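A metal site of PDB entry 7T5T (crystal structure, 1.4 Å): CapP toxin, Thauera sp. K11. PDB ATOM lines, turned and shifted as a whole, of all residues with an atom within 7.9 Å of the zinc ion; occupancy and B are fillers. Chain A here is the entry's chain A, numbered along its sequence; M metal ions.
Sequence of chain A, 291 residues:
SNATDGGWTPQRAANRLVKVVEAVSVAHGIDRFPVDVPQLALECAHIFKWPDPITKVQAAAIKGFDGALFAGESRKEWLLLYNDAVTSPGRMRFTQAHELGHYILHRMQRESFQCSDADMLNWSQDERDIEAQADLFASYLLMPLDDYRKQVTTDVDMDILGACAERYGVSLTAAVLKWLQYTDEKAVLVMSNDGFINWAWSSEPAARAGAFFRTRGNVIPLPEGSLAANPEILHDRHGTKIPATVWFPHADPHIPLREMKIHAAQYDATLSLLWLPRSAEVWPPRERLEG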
ATOM      1  N   GLY A  67      -0.460  12.650  14.122  1.00  0.00           N
ATOM      2  CA  GLY A  67      -1.359  12.893  15.251  1.00  0.00           C
ATOM      3  C   GLY A  67      -2.090  14.199  15.077  1.00  0.00           C
ATOM      4  O   GLY A  67      -1.677  15.051  14.285  1.00  0.00           O
ATOM      5  N   ALA A  68      -3.163  14.355  15.822  1.00  0.00           N
ATOM      6  CA  ALA A  68      -3.957  15.577  15.724  1.00  0.00           C
ATOM      7  C   ALA A  68      -4.732  15.770  17.012  1.00  0.00           C
ATOM      8  O   ALA A  68      -4.991  14.827  17.766  1.00  0.00           O
ATOM      9  CB  ALA A  68      -4.932  15.559  14.547  1.00  0.00           C
ATOM     10  N   LEU A  69      -5.078  17.032  17.251  1.00  0.00           N
ATOM     11  CA  LEU A  69      -5.929  17.453  18.353  1.00  0.00           C
ATOM     12  C   LEU A  69      -6.931  18.431  17.756  1.00  0.00           C
ATOM     13  O   LEU A  69      -6.549  19.475  17.240  1.00  0.00           O
ATOM     14  CB  LEU A  69      -5.085  18.125  19.426  1.00  0.00           C
ATOM     15  CG  LEU A  69      -5.873  18.521  20.681  1.00  0.00           C
ATOM     16  CD1 LEU A  69      -6.209  17.259  21.535  1.00  0.00           C
ATOM     17  CD2 LEU A  69      -5.107  19.542  21.488  1.00  0.00           C
ATOM     18  N   THR A  95       3.346  10.191  20.003  1.00  0.00           N
ATOM     19  CA  THR A  95       2.374  11.072  19.358  1.00  0.00           C
ATOM     20  C   THR A  95       1.264  11.455  20.308  1.00  0.00           C
ATOM     21  O   THR A  95       0.850  12.618  20.341  1.00  0.00           O
ATOM     22  CB  THR A  95       1.820  10.398  18.098  1.00  0.00           C
ATOM     23  OG1 THR A  95       2.858  10.361  17.126  1.00  0.00           O
ATOM     24  CG2 THR A  95       0.614  11.109  17.543  1.00  0.00           C
ATOM     25  N   HIS A  98       2.626  13.976  22.693  1.00  0.00           N
ATOM     26  CA  HIS A  98       2.843  15.232  21.980  1.00  0.00           C
ATOM     27  C   HIS A  98       1.543  16.006  21.830  1.00  0.00           C
ATOM     28  O   HIS A  98       1.493  17.216  22.123  1.00  0.00           O
ATOM     29  CB  HIS A  98       3.446  14.902  20.619  1.00  0.00           C
ATOM     30  CG  HIS A  98       3.585  16.079  19.691  1.00  0.00           C
ATOM     31  ND1 HIS A  98       4.790  16.684  19.446  1.00  0.00           N
ATOM     32  CD2 HIS A  98       2.680  16.706  18.901  1.00  0.00           C
ATOM     33  CE1 HIS A  98       4.625  17.635  18.546  1.00  0.00           C
ATOM     34  NE2 HIS A  98       3.351  17.664  18.190  1.00  0.00           N
ATOM     35  N   GLU A  99       0.466  15.326  21.418  1.00  0.00           N
ATOM     36  CA  GLU A  99      -0.826  16.003  21.282  1.00  0.00           C
ATOM     37  C   GLU A  99      -1.361  16.448  22.638  1.00  0.00           C
ATOM     38  O   GLU A  99      -1.956  17.528  22.760  1.00  0.00           O
ATOM     39  CB  GLU A  99      -1.845  15.120  20.585  1.00  0.00           C
ATOM     40  CG  GLU A  99      -1.499  14.736  19.157  1.00  0.00           C
ATOM     41  CD  GLU A  99      -1.221  15.931  18.248  1.00  0.00           C
ATOM     42  OE1 GLU A  99      -1.783  17.023  18.489  1.00  0.00           O
ATOM     43  OE2 GLU A  99      -0.432  15.781  17.283  1.00  0.00           O
ATOM     44  N   GLY A 101       0.515  17.442  24.990  1.00  0.00           N
ATOM     45  CA  GLY A 101       1.272  18.674  25.191  1.00  0.00           C
ATOM     46  C   GLY A 101       0.606  19.878  24.536  1.00  0.00           C
ATOM     47  O   GLY A 101       0.519  20.948  25.143  1.00  0.00           O
ATOM     48  N   HIS A 102       0.120  19.731  23.305  1.00  0.00           N
ATOM     49  CA  HIS A 102      -0.605  20.842  22.684  1.00  0.00           C
ATOM     50  C   HIS A 102      -1.849  21.188  23.476  1.00  0.00           C
ATOM     51  O   HIS A 102      -2.177  22.364  23.661  1.00  0.00           O
ATOM     52  CB  HIS A 102      -1.003  20.540  21.239  1.00  0.00           C
ATOM     53  CG  HIS A 102       0.131  20.546  20.265  1.00  0.00           C
ATOM     54  ND1 HIS A 102       1.140  21.475  20.270  1.00  0.00           N
ATOM     55  CD2 HIS A 102       0.371  19.742  19.194  1.00  0.00           C
ATOM     56  CE1 HIS A 102       1.960  21.243  19.266  1.00  0.00           C
ATOM     57  NE2 HIS A 102       1.516  20.200  18.594  1.00  0.00           N
ATOM     58  N   HIS A 106      -0.928  24.823  24.449  1.00  0.00           N
ATOM     59  CA  HIS A 106      -1.116  25.634  23.255  1.00  0.00           C
ATOM     60  C   HIS A 106      -2.558  25.760  22.771  1.00  0.00           C
ATOM     61  O   HIS A 106      -2.804  26.486  21.803  1.00  0.00           O
ATOM     62  CB  HIS A 106      -0.291  25.044  22.091  1.00  0.00           C
ATOM     63  CG  HIS A 106       1.137  24.775  22.454  1.00  0.00           C
ATOM     64  ND1 HIS A 106       1.760  23.578  22.192  1.00  0.00           N
ATOM     65  CD2 HIS A 106       2.051  25.555  23.064  1.00  0.00           C
ATOM     66  CE1 HIS A 106       3.004  23.633  22.641  1.00  0.00           C
ATOM     67  NE2 HIS A 106       3.204  24.823  23.176  1.00  0.00           N
ATOM     68  N   ARG A 110      -5.095  27.935  18.801  1.00  0.00           N
ATOM     69  CA  ARG A 110      -5.570  27.396  17.535  1.00  0.00           C
ATOM     70  C   ARG A 110      -6.842  26.601  17.773  1.00  0.00           C
ATOM     71  O   ARG A 110      -7.174  26.232  18.898  1.00  0.00           O
ATOM     72  CB  ARG A 110      -4.547  26.446  16.903  1.00  0.00           C
ATOM     73  CG  ARG A 110      -3.196  27.070  16.683  1.00  0.00           C
ATOM     74  CD  ARG A 110      -2.274  26.171  15.884  1.00  0.00           C
ATOM     75  NE  ARG A 110      -0.927  26.723  15.823  1.00  0.00           N
ATOM     76  CZ  ARG A 110       0.099  26.125  15.221  1.00  0.00           C
ATOM     77  NH1 ARG A 110      -0.032  24.960  14.630  1.00  0.00           N
ATOM     78  NH2 ARG A 110       1.292  26.718  15.239  1.00  0.00           N
ATOM     79  N   PHE A 113      -4.671  21.091  15.759  1.00  0.00           N
ATOM     80  CA  PHE A 113      -3.271  20.799  15.516  1.00  0.00           C
ATOM     81  C   PHE A 113      -3.203  19.517  14.710  1.00  0.00           C
ATOM     82  O   PHE A 113      -3.844  18.535  15.066  1.00  0.00           O
ATOM     83  CB  PHE A 113      -2.510  20.608  16.856  1.00  0.00           C
ATOM     84  CG  PHE A 113      -2.639  21.776  17.799  1.00  0.00           C
ATOM     85  CD1 PHE A 113      -3.775  21.928  18.574  1.00  0.00           C
ATOM     86  CD2 PHE A 113      -1.636  22.717  17.876  1.00  0.00           C
ATOM     87  CE1 PHE A 113      -3.913  23.023  19.403  1.00  0.00           C
ATOM     88  CE2 PHE A 113      -1.767  23.814  18.711  1.00  0.00           C
ATOM     89  CZ  PHE A 113      -2.907  23.967  19.463  1.00  0.00           C
ATOM     90  N   GLN A 114      -2.397  19.499  13.646  1.00  0.00           N
ATOM     91  CA  GLN A 114      -2.104  18.310  12.872  1.00  0.00           C
ATOM     92  C   GLN A 114      -0.591  18.242  12.737  1.00  0.00           C
ATOM     93  O   GLN A 114       0.030  19.206  12.280  1.00  0.00           O
ATOM     94  CB  GLN A 114      -2.757  18.399  11.496  1.00  0.00           C
ATOM     95  CG  GLN A 114      -4.265  18.311  11.563  1.00  0.00           C
ATOM     96  CD  GLN A 114      -4.961  18.846  10.322  1.00  0.00           C
ATOM     97  OE1 GLN A 114      -5.866  19.666  10.417  1.00  0.00           O
ATOM     98  NE2 GLN A 114      -4.510  18.423   9.164  1.00  0.00           N
ATOM     99  N   CYS A 115      -0.010  17.100  13.112  1.00  0.00           N
ATOM    100  CA  CYS A 115       1.420  17.014  13.405  1.00  0.00           C
ATOM    101  C   CYS A 115       2.033  15.808  12.726  1.00  0.00           C
ATOM    102  O   CYS A 115       1.499  14.699  12.816  1.00  0.00           O
ATOM    103  CB  CYS A 115       1.644  16.928  14.918  1.00  0.00           C
ATOM    104  SG  CYS A 115       0.759  18.220  15.831  1.00  0.00           S
ATOM    105  N   SER A 116       3.138  16.045  12.018  1.00  0.00           N
ATOM    106  CA  SER A 116       3.793  15.018  11.232  1.00  0.00           C
ATOM    107  C   SER A 116       4.887  14.291  12.035  1.00  0.00           C
ATOM    108  O   SER A 116       5.288  14.719  13.117  1.00  0.00           O
ATOM    109  CB  SER A 116       4.472  15.664  10.043  1.00  0.00           C
ATOM    110  OG  SER A 116       5.522  16.518  10.497  1.00  0.00           O
ATOM    111  N   ASP A 119       7.509  16.666  12.918  1.00  0.00           N
ATOM    112  CA  ASP A 119       7.225  17.439  14.120  1.00  0.00           C
ATOM    113  C   ASP A 119       7.641  16.674  15.368  1.00  0.00           C
ATOM    114  O   ASP A 119       8.086  17.289  16.341  1.00  0.00           O
ATOM    115  CB  ASP A 119       5.743  17.791  14.177  1.00  0.00           C
ATOM    116  CG  ASP A 119       5.326  18.793  13.099  1.00  0.00           C
ATOM    117  OD1 ASP A 119       6.138  19.692  12.755  1.00  0.00           O
ATOM    118  OD2 ASP A 119       4.154  18.690  12.635  1.00  0.00           O
ATOM    119  N   MET A 120       7.510  15.350  15.366  1.00  0.00           N
ATOM    120  CA  MET A 120       7.833  14.552  16.541  1.00  0.00           C
ATOM    121  C   MET A 120       9.341  14.400  16.735  1.00  0.00           C
ATOM    122  O   MET A 120       9.765  14.005  17.810  1.00  0.00           O
ATOM    123  CB  MET A 120       7.249  13.146  16.425  1.00  0.00           C
ATOM    124  CG  MET A 120       5.796  13.063  16.094  1.00  0.00           C
ATOM    125  SD  MET A 120       4.766  13.896  17.327  1.00  0.00           S
ATOM    126  CE  MET A 120       3.187  13.900  16.499  1.00  0.00           C
ATOM    127  N   ASP A 129       8.742  27.571  19.352  1.00  0.00           N
ATOM    128  CA  ASP A 129       8.452  26.468  18.439  1.00  0.00           C
ATOM    129  C   ASP A 129       7.514  25.533  19.172  1.00  0.00           C
ATOM    130  O   ASP A 129       7.944  24.756  20.036  1.00  0.00           O
ATOM    131  CB  ASP A 129       9.754  25.780  18.042  1.00  0.00           C
ATOM    132  CG  ASP A 129       9.563  24.678  17.037  1.00  0.00           C
ATOM    133  OD1 ASP A 129       8.441  24.124  16.972  1.00  0.00           O
ATOM    134  OD2 ASP A 129      10.530  24.356  16.289  1.00  0.00           O
ATOM    135  N   ILE A 130       6.221  25.590  18.841  1.00  0.00           N
ATOM    136  CA  ILE A 130       5.271  24.809  19.635  1.00  0.00           C
ATOM    137  C   ILE A 130       5.428  23.317  19.429  1.00  0.00           C
ATOM    138  O   ILE A 130       5.016  22.541  20.288  1.00  0.00           O
ATOM    139  CB  ILE A 130       3.791  25.232  19.480  1.00  0.00           C
ATOM    140  CG1 ILE A 130       3.259  24.950  18.100  1.00  0.00           C
ATOM    141  CG2 ILE A 130       3.645  26.694  19.848  1.00  0.00           C
ATOM    142  CD1 ILE A 130       1.740  25.016  18.033  1.00  0.00           C
ATOM    143  N   GLU A 131       5.946  22.897  18.264  1.00  0.00           N
ATOM    144  CA  GLU A 131       6.188  21.484  18.031  1.00  0.00           C
ATOM    145  C   GLU A 131       7.319  20.988  18.914  1.00  0.00           C
ATOM    146  O   GLU A 131       7.189  19.937  19.556  1.00  0.00           O
ATOM    147  CB  GLU A 131       6.467  21.209  16.558  1.00  0.00           C
ATOM    148  CG  GLU A 131       5.367  21.685  15.623  1.00  0.00           C
ATOM    149  CD  GLU A 131       4.003  21.115  15.980  1.00  0.00           C
ATOM    150  OE1 GLU A 131       3.932  19.920  16.364  1.00  0.00           O
ATOM    151  OE2 GLU A 131       2.997  21.843  15.843  1.00  0.00           O
ATOM    152  N   ALA A 132       8.409  21.742  18.978  1.00  0.00           N
ATOM    153  CA  ALA A 132       9.491  21.421  19.895  1.00  0.00           C
ATOM    154  C   ALA A 132       9.005  21.406  21.334  1.00  0.00           C
ATOM    155  O   ALA A 132       9.364  20.510  22.096  1.00  0.00           O
ATOM    156  CB  ALA A 132      10.632  22.420  19.707  1.00  0.00           C
ATOM    157  N   ALA A 134       5.960  20.753  22.486  1.00  0.00           N
ATOM    158  CA  ALA A 134       5.186  19.536  22.699  1.00  0.00           C
ATOM    159  C   ALA A 134       6.081  18.300  22.774  1.00  0.00           C
ATOM    160  O   ALA A 134       5.809  17.398  23.586  1.00  0.00           O
ATOM    161  CB  ALA A 134       4.121  19.389  21.634  1.00  0.00           C
ATOM    162  N   ASP A 135       7.157  18.277  21.999  1.00  0.00           N
ATOM    163  CA  ASP A 135       8.128  17.179  22.097  1.00  0.00           C
ATOM    164  C   ASP A 135       8.822  17.167  23.446  1.00  0.00           C
ATOM    165  O   ASP A 135       9.022  16.098  24.035  1.00  0.00           O
ATOM    166  CB  ASP A 135       9.173  17.312  20.983  1.00  0.00           C
ATOM    167  CG  ASP A 135       8.613  17.042  19.613  1.00  0.00           C
ATOM    168  OD1 ASP A 135       7.557  16.395  19.507  1.00  0.00           O
ATOM    169  OD2 ASP A 135       9.293  17.453  18.627  1.00  0.00           O
HETATM  170 ZN    ZN M   1       2.391  19.099  17.108  1.00  0.00          ZN
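The zinc ion is bound by the side-chain carboxylate of Glu 131, a ring nitrogen (NE2) of His 98, a ring nitrogen (NE2) of His 102 and the side-chain sulfur of Cys 115.
Four residues have an atom within 4 Å of the zinc ion: His 98, His 102, Cys 115 and Glu 131.
The nearest printed residue that does not touch the zinc ion is Glu 99 (4.4 Å).
The backbone NH (N) of Glu 131 sits at hydrogen-bond distance from the side-chain carboxylate (OD1) of Asp 129, 3.1 Å away.
ND1 of His 98 lies close to SD of Met 120 (3.5 Å).
A ring nitrogen (ND1) of His 98 sits at hydrogen-bond distance from the side-chain carboxylate of Asp 135, 2.8 Å away.
A ring nitrogen (ND1) of His 102 sits at hydrogen-bond distance from a ring nitrogen (ND1) of His 106 (2.9 Å).
The side-chain sulfur (SG) of Cys 115 sits close to the side-chain carboxylate (OE2) of Glu 99 (3.1 Å).
The backbone NH (N) of Cys 115 is in hydrogen-bond range of the backbone carbonyl oxygen (O) of Gly 67 (2.9 Å).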
